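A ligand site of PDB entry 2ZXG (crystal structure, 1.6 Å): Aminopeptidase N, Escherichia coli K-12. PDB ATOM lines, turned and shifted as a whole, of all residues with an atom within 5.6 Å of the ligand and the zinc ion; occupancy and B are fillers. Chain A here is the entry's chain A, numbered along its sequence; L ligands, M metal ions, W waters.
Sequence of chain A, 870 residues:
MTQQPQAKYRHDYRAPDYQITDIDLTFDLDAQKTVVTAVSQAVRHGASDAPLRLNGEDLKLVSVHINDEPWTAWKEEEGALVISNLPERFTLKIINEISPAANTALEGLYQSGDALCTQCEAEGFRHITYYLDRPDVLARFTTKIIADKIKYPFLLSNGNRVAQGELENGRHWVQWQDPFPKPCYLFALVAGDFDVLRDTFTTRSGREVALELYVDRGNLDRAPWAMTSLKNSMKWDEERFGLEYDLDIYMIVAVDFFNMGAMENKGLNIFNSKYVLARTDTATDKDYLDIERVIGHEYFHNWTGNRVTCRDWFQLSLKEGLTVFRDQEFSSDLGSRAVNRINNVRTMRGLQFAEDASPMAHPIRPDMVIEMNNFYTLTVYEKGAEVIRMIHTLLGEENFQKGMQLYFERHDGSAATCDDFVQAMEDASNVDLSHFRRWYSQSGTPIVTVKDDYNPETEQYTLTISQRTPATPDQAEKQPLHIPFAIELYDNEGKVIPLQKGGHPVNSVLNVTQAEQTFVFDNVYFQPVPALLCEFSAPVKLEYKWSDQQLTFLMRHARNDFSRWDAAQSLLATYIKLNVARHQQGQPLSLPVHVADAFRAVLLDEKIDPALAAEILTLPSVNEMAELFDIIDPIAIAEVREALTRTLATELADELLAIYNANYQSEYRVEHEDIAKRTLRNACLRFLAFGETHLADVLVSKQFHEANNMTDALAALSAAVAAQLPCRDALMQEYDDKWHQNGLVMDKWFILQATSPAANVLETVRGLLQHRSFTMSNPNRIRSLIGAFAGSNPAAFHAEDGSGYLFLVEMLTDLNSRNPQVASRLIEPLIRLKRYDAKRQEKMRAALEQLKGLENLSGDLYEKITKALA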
ATOM      1  N   GLN A 119       8.490 -27.673  -0.998  1.00  0.00           N
ATOM      2  CA  GLN A 119       8.527 -26.845  -2.186  1.00  0.00           C
ATOM      3  C   GLN A 119       8.352 -27.775  -3.386  1.00  0.00           C
ATOM      4  O   GLN A 119       9.191 -28.662  -3.596  1.00  0.00           O
ATOM      5  CB  GLN A 119       9.838 -26.083  -2.289  1.00  0.00           C
ATOM      6  CG  GLN A 119       9.998 -25.319  -3.635  1.00  0.00           C
ATOM      7  CD  GLN A 119       8.851 -24.355  -3.890  1.00  0.00           C
ATOM      8  OE1 GLN A 119       8.268 -23.806  -2.950  1.00  0.00           O
ATOM      9  NE2 GLN A 119       8.522 -24.133  -5.155  1.00  0.00           N
ATOM     10  N   GLU A 121       7.214 -26.573  -6.776  1.00  0.00           N
ATOM     11  CA  GLU A 121       7.435 -26.020  -8.131  1.00  0.00           C
ATOM     12  C   GLU A 121       8.938 -26.039  -8.442  1.00  0.00           C
ATOM     13  O   GLU A 121       9.743 -25.647  -7.604  1.00  0.00           O
ATOM     14  CB  GLU A 121       6.889 -24.592  -8.255  1.00  0.00           C
ATOM     15  CG  GLU A 121       6.937 -24.096  -9.688  1.00  0.00           C
ATOM     16  CD  GLU A 121       6.376 -22.709  -9.873  1.00  0.00           C
ATOM     17  OE1 GLU A 121       6.330 -22.245 -11.032  1.00  0.00           O
ATOM     18  OE2 GLU A 121       5.966 -22.063  -8.887  1.00  0.00           O
ATOM     19  N   ASN A 259      14.464 -21.924  -1.250  1.00  0.00           N
ATOM     20  CA  ASN A 259      15.233 -21.628  -2.489  1.00  0.00           C
ATOM     21  C   ASN A 259      14.620 -20.567  -3.393  1.00  0.00           C
ATOM     22  O   ASN A 259      15.085 -20.341  -4.525  1.00  0.00           O
ATOM     23  CB  ASN A 259      15.375 -22.899  -3.332  1.00  0.00           C
ATOM     24  CG  ASN A 259      16.406 -23.856  -2.808  1.00  0.00           C
ATOM     25  OD1 ASN A 259      17.233 -23.513  -1.972  1.00  0.00           O
ATOM     26  ND2 ASN A 259      16.356 -25.082  -3.311  1.00  0.00           N
ATOM     27  N   MET A 260      13.541 -19.945  -2.965  1.00  0.00           N
ATOM     28  CA  MET A 260      12.988 -18.830  -3.741  1.00  0.00           C
ATOM     29  C   MET A 260      12.460 -17.815  -2.769  1.00  0.00           C
ATOM     30  O   MET A 260      12.636 -17.948  -1.547  1.00  0.00           O
ATOM     31  CB  MET A 260      11.915 -19.301  -4.718  1.00  0.00           C
ATOM     32  CG  MET A 260      10.741 -20.031  -4.083  1.00  0.00           C
ATOM     33  SD  MET A 260       9.542 -20.757  -5.254  1.00  0.00           S
ATOM     34  CE  MET A 260      10.633 -21.756  -6.258  1.00  0.00           C
ATOM     35  N   GLY A 261      11.855 -16.761  -3.295  1.00  0.00           N
ATOM     36  CA  GLY A 261      11.342 -15.711  -2.437  1.00  0.00           C
ATOM     37  C   GLY A 261      10.091 -16.156  -1.743  1.00  0.00           C
ATOM     38  O   GLY A 261       9.908 -15.868  -0.561  1.00  0.00           O
ATOM     39  N   ALA A 262       9.215 -16.841  -2.478  1.00  0.00           N
ATOM     40  CA  ALA A 262       7.910 -17.236  -1.940  1.00  0.00           C
ATOM     41  C   ALA A 262       7.200 -18.100  -2.972  1.00  0.00           C
ATOM     42  O   ALA A 262       7.683 -18.226  -4.091  1.00  0.00           O
ATOM     43  CB  ALA A 262       7.074 -15.977  -1.593  1.00  0.00           C
ATOM     44  N   MET A 263       6.075 -18.704  -2.585  1.00  0.00           N
ATOM     45  CA  MET A 263       5.431 -19.692  -3.433  1.00  0.00           C
ATOM     46  C   MET A 263       3.935 -19.688  -3.227  1.00  0.00           C
ATOM     47  O   MET A 263       3.460 -19.736  -2.073  1.00  0.00           O
ATOM     48  CB  MET A 263       6.026 -21.078  -3.152  1.00  0.00           C
ATOM     49  CG  MET A 263       5.366 -22.197  -3.942  1.00  0.00           C
ATOM     50  SD  MET A 263       5.701 -22.013  -5.732  1.00  0.00           S
ATOM     51  CE  MET A 263       4.156 -22.671  -6.362  1.00  0.00           C
ATOM     52  N   GLU A 264       3.205 -19.650  -4.340  1.00  0.00           N
ATOM     53  CA  GLU A 264       1.750 -19.440  -4.338  1.00  0.00           C
ATOM     54  C   GLU A 264       0.895 -20.680  -4.073  1.00  0.00           C
ATOM     55  O   GLU A 264      -0.226 -20.749  -4.584  1.00  0.00           O
ATOM     56  CB  GLU A 264       1.323 -18.793  -5.662  1.00  0.00           C
ATOM     57  CG  GLU A 264       1.462 -19.713  -6.914  1.00  0.00           C
ATOM     58  CD  GLU A 264       2.812 -19.613  -7.627  1.00  0.00           C
ATOM     59  OE1 GLU A 264       2.849 -19.959  -8.835  1.00  0.00           O
ATOM     60  OE2 GLU A 264       3.819 -19.214  -7.005  1.00  0.00           O
ATOM     61  N   TYR A 275      10.810 -12.124   2.957  1.00  0.00           N
ATOM     62  CA  TYR A 275       9.697 -11.419   2.347  1.00  0.00           C
ATOM     63  C   TYR A 275       8.461 -11.414   3.244  1.00  0.00           C
ATOM     64  O   TYR A 275       7.353 -11.188   2.776  1.00  0.00           O
ATOM     65  CB  TYR A 275       9.414 -11.972   0.942  1.00  0.00           C
ATOM     66  CG  TYR A 275      10.528 -11.661  -0.028  1.00  0.00           C
ATOM     67  CD1 TYR A 275      10.926 -10.340  -0.256  1.00  0.00           C
ATOM     68  CD2 TYR A 275      11.199 -12.674  -0.694  1.00  0.00           C
ATOM     69  CE1 TYR A 275      11.945 -10.040  -1.132  1.00  0.00           C
ATOM     70  CE2 TYR A 275      12.219 -12.377  -1.597  1.00  0.00           C
ATOM     71  CZ  TYR A 275      12.587 -11.063  -1.806  1.00  0.00           C
ATOM     72  OH  TYR A 275      13.604 -10.749  -2.683  1.00  0.00           O
ATOM     73  N   ARG A 293       5.501  -6.074  -2.231  1.00  0.00           N
ATOM     74  CA  ARG A 293       5.403  -6.552  -3.594  1.00  0.00           C
ATOM     75  C   ARG A 293       5.364  -8.072  -3.677  1.00  0.00           C
ATOM     76  O   ARG A 293       4.688  -8.588  -4.554  1.00  0.00           O
ATOM     77  CB  ARG A 293       6.516  -5.942  -4.465  1.00  0.00           C
ATOM     78  CG  ARG A 293       7.757  -6.760  -4.585  1.00  0.00           C
ATOM     79  CD  ARG A 293       8.786  -6.043  -5.483  1.00  0.00           C
ATOM     80  NE  ARG A 293       9.462  -4.963  -4.753  1.00  0.00           N
ATOM     81  CZ  ARG A 293       9.236  -3.659  -4.927  1.00  0.00           C
ATOM     82  NH1 ARG A 293       8.353  -3.221  -5.816  1.00  0.00           N
ATOM     83  NH2 ARG A 293       9.922  -2.777  -4.196  1.00  0.00           N
ATOM     84  N   VAL A 294       6.060  -8.781  -2.786  1.00  0.00           N
ATOM     85  CA  VAL A 294       6.077 -10.254  -2.841  1.00  0.00           C
ATOM     86  C   VAL A 294       4.797 -10.828  -2.245  1.00  0.00           C
ATOM     87  O   VAL A 294       4.215 -11.771  -2.802  1.00  0.00           O
ATOM     88  CB  VAL A 294       7.353 -10.850  -2.200  1.00  0.00           C
ATOM     89  CG1 VAL A 294       7.310 -12.379  -2.212  1.00  0.00           C
ATOM     90  CG2 VAL A 294       8.588 -10.377  -2.976  1.00  0.00           C
ATOM     91  N   HIS A 297       2.517 -10.296  -5.067  1.00  0.00           N
ATOM     92  CA  HIS A 297       2.807 -11.264  -6.122  1.00  0.00           C
ATOM     93  C   HIS A 297       2.147 -12.629  -5.842  1.00  0.00           C
ATOM     94  O   HIS A 297       1.452 -13.180  -6.697  1.00  0.00           O
ATOM     95  CB  HIS A 297       4.326 -11.430  -6.230  1.00  0.00           C
ATOM     96  CG  HIS A 297       4.785 -12.290  -7.360  1.00  0.00           C
ATOM     97  ND1 HIS A 297       5.210 -11.766  -8.566  1.00  0.00           N
ATOM     98  CD2 HIS A 297       4.919 -13.626  -7.467  1.00  0.00           C
ATOM     99  CE1 HIS A 297       5.567 -12.755  -9.373  1.00  0.00           C
ATOM    100  NE2 HIS A 297       5.406 -13.898  -8.724  1.00  0.00           N
ATOM    101  N   GLU A 298       2.375 -13.166  -4.638  1.00  0.00           N
ATOM    102  CA  GLU A 298       1.841 -14.479  -4.312  1.00  0.00           C
ATOM    103  C   GLU A 298       0.324 -14.449  -4.308  1.00  0.00           C
ATOM    104  O   GLU A 298      -0.321 -15.383  -4.819  1.00  0.00           O
ATOM    105  CB  GLU A 298       2.381 -14.991  -2.977  1.00  0.00           C
ATOM    106  CG  GLU A 298       3.910 -15.098  -2.968  1.00  0.00           C
ATOM    107  CD  GLU A 298       4.478 -15.878  -4.133  1.00  0.00           C
ATOM    108  OE1 GLU A 298       3.812 -16.813  -4.645  1.00  0.00           O
ATOM    109  OE2 GLU A 298       5.598 -15.531  -4.544  1.00  0.00           O
ATOM    110  N   HIS A 301      -1.024 -14.461  -7.864  1.00  0.00           N
ATOM    111  CA  HIS A 301      -0.962 -15.790  -8.480  1.00  0.00           C
ATOM    112  C   HIS A 301      -2.248 -16.591  -8.252  1.00  0.00           C
ATOM    113  O   HIS A 301      -2.509 -17.547  -8.986  1.00  0.00           O
ATOM    114  CB  HIS A 301       0.200 -16.603  -7.923  1.00  0.00           C
ATOM    115  CG  HIS A 301       1.492 -16.481  -8.683  1.00  0.00           C
ATOM    116  ND1 HIS A 301       1.578 -16.638 -10.045  1.00  0.00           N
ATOM    117  CD2 HIS A 301       2.763 -16.340  -8.239  1.00  0.00           C
ATOM    118  CE1 HIS A 301       2.848 -16.537 -10.414  1.00  0.00           C
ATOM    119  NE2 HIS A 301       3.580 -16.371  -9.337  1.00  0.00           N
ATOM    120  N   LYS A 319       2.109 -17.302 -16.392  1.00  0.00           N
ATOM    121  CA  LYS A 319       1.828 -16.884 -15.019  1.00  0.00           C
ATOM    122  C   LYS A 319       2.851 -15.901 -14.474  1.00  0.00           C
ATOM    123  O   LYS A 319       2.471 -14.995 -13.726  1.00  0.00           O
ATOM    124  CB  LYS A 319       1.613 -18.086 -14.078  1.00  0.00           C
ATOM    125  CG  LYS A 319       2.829 -18.933 -13.721  1.00  0.00           C
ATOM    126  CD  LYS A 319       2.359 -20.067 -12.764  1.00  0.00           C
ATOM    127  CE  LYS A 319       3.474 -21.005 -12.329  1.00  0.00           C
ATOM    128  NZ  LYS A 319       4.387 -20.435 -11.270  1.00  0.00           N
ATOM    129  N   GLU A 320       4.132 -16.047 -14.832  1.00  0.00           N
ATOM    130  CA  GLU A 320       5.145 -15.198 -14.179  1.00  0.00           C
ATOM    131  C   GLU A 320       5.241 -13.806 -14.786  1.00  0.00           C
ATOM    132  O   GLU A 320       5.318 -12.822 -14.029  1.00  0.00           O
ATOM    133  CB  GLU A 320       6.510 -15.870 -14.131  1.00  0.00           C
ATOM    134  CG  GLU A 320       6.529 -17.165 -13.331  1.00  0.00           C
ATOM    135  CD  GLU A 320       6.047 -17.007 -11.895  1.00  0.00           C
ATOM    136  OE1 GLU A 320       5.721 -18.031 -11.265  1.00  0.00           O
ATOM    137  OE2 GLU A 320       6.009 -15.861 -11.371  1.00  0.00           O
ATOM    138  N   THR A 323       1.999 -12.133 -13.602  1.00  0.00           N
ATOM    139  CA  THR A 323       1.973 -11.868 -12.160  1.00  0.00           C
ATOM    140  C   THR A 323       2.990 -10.798 -11.778  1.00  0.00           C
ATOM    141  O   THR A 323       2.707  -9.998 -10.881  1.00  0.00           O
ATOM    142  CB  THR A 323       2.121 -13.169 -11.338  1.00  0.00           C
ATOM    143  OG1 THR A 323       1.055 -14.064 -11.729  1.00  0.00           O
ATOM    144  CG2 THR A 323       2.030 -12.889  -9.844  1.00  0.00           C
ATOM    145  N   ASP A 327       2.219  -7.390  -9.894  1.00  0.00           N
ATOM    146  CA  ASP A 327       2.886  -6.870  -8.698  1.00  0.00           C
ATOM    147  C   ASP A 327       3.462  -5.472  -8.949  1.00  0.00           C
ATOM    148  O   ASP A 327       3.459  -4.638  -8.059  1.00  0.00           O
ATOM    149  CB  ASP A 327       3.859  -7.874  -8.017  1.00  0.00           C
ATOM    150  CG  ASP A 327       5.273  -7.929  -8.651  1.00  0.00           C
ATOM    151  OD1 ASP A 327       5.765  -9.067  -8.885  1.00  0.00           O
ATOM    152  OD2 ASP A 327       5.931  -6.874  -8.801  1.00  0.00           O
ATOM    153  N   TYR A 376      13.655 -19.964 -14.294  1.00  0.00           N
ATOM    154  CA  TYR A 376      12.975 -18.973 -13.449  1.00  0.00           C
ATOM    155  C   TYR A 376      13.797 -17.691 -13.521  1.00  0.00           C
ATOM    156  O   TYR A 376      14.454 -17.290 -12.572  1.00  0.00           O
ATOM    157  CB  TYR A 376      12.790 -19.539 -12.013  1.00  0.00           C
ATOM    158  CG  TYR A 376      11.658 -20.544 -12.037  1.00  0.00           C
ATOM    159  CD1 TYR A 376      11.846 -21.821 -12.607  1.00  0.00           C
ATOM    160  CD2 TYR A 376      10.381 -20.199 -11.587  1.00  0.00           C
ATOM    161  CE1 TYR A 376      10.793 -22.734 -12.683  1.00  0.00           C
ATOM    162  CE2 TYR A 376       9.327 -21.111 -11.649  1.00  0.00           C
ATOM    163  CZ  TYR A 376       9.552 -22.363 -12.197  1.00  0.00           C
ATOM    164  OH  TYR A 376       8.521 -23.257 -12.308  1.00  0.00           O
ATOM    165  N   TYR A 381      10.460 -13.673 -16.180  1.00  0.00           N
ATOM    166  CA  TYR A 381       9.797 -12.785 -15.213  1.00  0.00           C
ATOM    167  C   TYR A 381       9.713 -11.349 -15.693  1.00  0.00           C
ATOM    168  O   TYR A 381       8.622 -10.840 -15.996  1.00  0.00           O
ATOM    169  CB  TYR A 381      10.545 -12.840 -13.863  1.00  0.00           C
ATOM    170  CG  TYR A 381      10.164 -14.028 -13.018  1.00  0.00           C
ATOM    171  CD1 TYR A 381      10.512 -15.319 -13.399  1.00  0.00           C
ATOM    172  CD2 TYR A 381       9.464 -13.842 -11.824  1.00  0.00           C
ATOM    173  CE1 TYR A 381      10.130 -16.420 -12.611  1.00  0.00           C
ATOM    174  CE2 TYR A 381       9.101 -14.913 -11.037  1.00  0.00           C
ATOM    175  CZ  TYR A 381       9.441 -16.206 -11.447  1.00  0.00           C
ATOM    176  OH  TYR A 381       9.069 -17.279 -10.674  1.00  0.00           O
ATOM    177  N   GLU A 382      10.878 -10.684 -15.776  1.00  0.00           N
ATOM    178  CA  GLU A 382      10.901  -9.248 -16.043  1.00  0.00           C
ATOM    179  C   GLU A 382      10.658  -8.910 -17.511  1.00  0.00           C
ATOM    180  O   GLU A 382       9.848  -8.011 -17.804  1.00  0.00           O
ATOM    181  CB  GLU A 382      12.194  -8.618 -15.534  1.00  0.00           C
ATOM    182  CG  GLU A 382      12.149  -8.224 -14.060  1.00  0.00           C
ATOM    183  CD  GLU A 382      12.510  -9.333 -13.083  1.00  0.00           C
ATOM    184  OE1 GLU A 382      12.872 -10.457 -13.518  1.00  0.00           O
ATOM    185  OE2 GLU A 382      12.455  -9.057 -11.856  1.00  0.00           O
ATOM    186  N   GLN A 821      20.038 -26.012  -7.030  1.00  0.00           N
ATOM    187  CA  GLN A 821      19.319 -24.799  -7.447  1.00  0.00           C
ATOM    188  C   GLN A 821      20.085 -23.554  -7.036  1.00  0.00           C
ATOM    189  O   GLN A 821      20.245 -22.620  -7.827  1.00  0.00           O
ATOM    190  CB  GLN A 821      17.917 -24.746  -6.841  1.00  0.00           C
ATOM    191  CG  GLN A 821      16.895 -25.363  -7.704  1.00  0.00           C
ATOM    192  CD  GLN A 821      15.518 -25.229  -7.081  1.00  0.00           C
ATOM    193  OE1 GLN A 821      14.750 -24.317  -7.415  1.00  0.00           O
ATOM    194  NE2 GLN A 821      15.219 -26.124  -6.153  1.00  0.00           N
ATOM    195  N   ARG A 825      22.117 -20.664  -9.467  1.00  0.00           N
ATOM    196  CA  ARG A 825      22.007 -19.200  -9.368  1.00  0.00           C
ATOM    197  C   ARG A 825      23.405 -18.595  -9.262  1.00  0.00           C
ATOM    198  O   ARG A 825      23.700 -17.564  -9.888  1.00  0.00           O
ATOM    199  CB  ARG A 825      21.174 -18.783  -8.150  1.00  0.00           C
ATOM    200  CG  ARG A 825      19.702 -19.047  -8.306  1.00  0.00           C
ATOM    201  CD  ARG A 825      18.910 -18.325  -7.207  1.00  0.00           C
ATOM    202  NE  ARG A 825      18.581 -16.942  -7.578  1.00  0.00           N
ATOM    203  CZ  ARG A 825      17.921 -16.088  -6.786  1.00  0.00           C
ATOM    204  NH1 ARG A 825      17.528 -16.454  -5.575  1.00  0.00           N
ATOM    205  NH2 ARG A 825      17.664 -14.863  -7.225  1.00  0.00           N
HETATM  206  O1  LIG L   1       6.190 -16.780  -6.760  1.00  0.00           O
HETATM  207  P1  LIG L   1       7.329 -17.272  -7.471  1.00  0.00           P
HETATM  208  O2  LIG L   1       7.226 -16.689  -8.806  1.00  0.00           O
HETATM  209  C1  LIG L   1       7.196 -18.871  -7.611  1.00  0.00           C
HETATM  210  N1  LIG L   1       6.084 -19.326  -8.441  1.00  0.00           N
HETATM  211  C2  LIG L   1       8.411 -19.580  -8.230  1.00  0.00           C
HETATM  212  C3  LIG L   1       8.713 -16.879  -6.782  1.00  0.00           C
HETATM  213  C4  LIG L   1       9.206 -15.408  -6.867  1.00  0.00           C
HETATM  214  C5  LIG L   1       8.654 -14.522  -5.716  1.00  0.00           C
HETATM  215  C6  LIG L   1       9.093 -13.075  -5.901  1.00  0.00           C
HETATM  216  C7  LIG L   1       8.291 -12.203  -6.654  1.00  0.00           C
HETATM  217  C8  LIG L   1       8.676 -10.879  -6.841  1.00  0.00           C
HETATM  218  C9  LIG L   1       9.876 -10.435  -6.295  1.00  0.00           C
HETATM  219  C10 LIG L   1      10.698 -11.285  -5.550  1.00  0.00           C
HETATM  220  C11 LIG L   1      10.301 -12.615  -5.342  1.00  0.00           C
HETATM  221  C12 LIG L   1      10.725 -15.255  -6.898  1.00  0.00           C
HETATM  222  O3  LIG L   1      11.435 -15.672  -5.993  1.00  0.00           O
HETATM  223  N2  LIG L   1      11.225 -14.610  -7.959  1.00  0.00           N
HETATM  224  C13 LIG L   1      12.611 -14.162  -8.042  1.00  0.00           C
HETATM  225  C14 LIG L   1      12.668 -12.741  -8.519  1.00  0.00           C
HETATM  226  O4  LIG L   1      13.612 -12.021  -8.123  1.00  0.00           O
HETATM  227  O5  LIG L   1      11.779 -12.322  -9.293  1.00  0.00           O
HETATM  228  C15 LIG L   1      13.423 -15.043  -9.000  1.00  0.00           C
HETATM  229  C16 LIG L   1      13.490 -16.483  -8.563  1.00  0.00           C
HETATM  230  C17 LIG L   1      14.493 -16.903  -7.683  1.00  0.00           C
HETATM  231  C18 LIG L   1      14.568 -18.246  -7.281  1.00  0.00           C
HETATM  232  C19 LIG L   1      13.629 -19.170  -7.761  1.00  0.00           C
HETATM  233  C20 LIG L   1      12.604 -18.743  -8.623  1.00  0.00           C
HETATM  234  C21 LIG L   1      12.541 -17.400  -9.038  1.00  0.00           C
HETATM  235 ZN    ZN M   1       5.544 -15.794  -9.458  1.00  0.00          ZN
HETATM  236  O   HOH W   1      13.355 -12.369 -11.700  1.00  0.00           O
HETATM  237  O   HOH W   2      10.352 -10.202 -10.048  1.00  0.00           O
HETATM  238  O   HOH W   3      15.212 -14.552 -11.930  1.00  0.00           O
HETATM  239  O   HOH W   4      13.913 -14.575  -4.351  1.00  0.00           O
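OE2 of Glu 320 is bound to the zinc ion (2.0 Å). O2 of the ligand binds the zinc ion (2.0 Å). The zinc ion is bound by NE2 of His 297, at 2.0 Å. The zinc ion is bound by NE2 of His 301.
N of Glu 264 lies within hydrogen-bond range of OE1 of Glu 298, at 2.9 Å. The side-chain hydroxyl (OH) of Tyr 376 sits at hydrogen-bond distance from the side-chain carboxylate (OE1) of Glu 121, at 2.7 Å. The side-chain carboxylate (OE1) of Glu 121 lies within salt-bridge range of the side-chain amino group (NZ) of Lys 319 (2.7 Å). NE2 of Gln 119 lies within hydrogen-bond range of SD of Met 263 (3.6 Å). ND2 of Asn 259 lies close to NE2 of Gln 821 (3.2 Å). The side-chain amino group (NZ) of Lys 319 is in salt-bridge range of the side-chain carboxylate (OE1) of Glu 320 (2.7 Å). A ring nitrogen (ND1) of His 301 is in hydrogen-bond range of the side-chain hydroxyl (OG1) of Thr 323 (3.1 Å). ND1 of His 297 lies within hydrogen-bond range of OD1 of Asp 327, at 2.8 Å.
Tyr 381 touches the zinc ion. Four residues have an atom within 4 Å of the zinc ion: His 297, His 301, Glu 320 and Tyr 381. The nearest printed residue that does not touch the zinc ion is Glu 264 (4.5 Å).
A nitrogen (N1) of the ligand sits close to the side-chain amino group (NZ) of Lys 319. The side-chain carboxylate (OE2) of Glu 121 lies within salt-bridge range of a nitrogen (N1) of the ligand, at 2.8 Å. The side-chain hydroxyl (OH) of Tyr 381 lies close to an oxygen (O2) of the ligand. N1 of the ligand lies within salt-bridge range of OE2 of Glu 264, at 2.7 Å. N of Gly 261 is in hydrogen-bond range of O3 of the ligand. OE2 of Glu 298 sits close to O1 of the ligand (2.6 Å).
An oxygen (O1) of the ligand lies close to the backbone carbonyl oxygen (O) of Ala 262 (3.4 Å). Asn 259 touches the ligand (O to C18, 3.5 Å). Met 260 touches the ligand. Met 263 touches the ligand. CG2 of Val 294 touches C10 of the ligand (3.4 Å). Asp 327 touches the ligand (OD1 to C8, 3.99 Å). CB of Tyr 376 touches C20 of the ligand (3.5 Å). Arg 825 touches the ligand. 17 residues have an atom within 4 Å of the ligand: Glu 121, Asn 259, Met 260, Gly 261, Ala 262, Met 263, Glu 264, Val 294, His 297, Glu 298, His 301, Lys 319, Glu 320, Asp 327, Tyr 376, Tyr 381 and Arg 825.
Water W2 bridges O5 of the ligand (2.7 Å) and OE2 of Glu 382 (3.0 Å). Water W1 bridges OE1 of Glu 382 (2.7 Å) and O5 of the ligand (2.9 Å). Water W4 lies within hydrogen-bond range of an oxygen (O3) of the ligand (3.2 Å) and the backbone NH of Gly 261 (3.2 Å).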
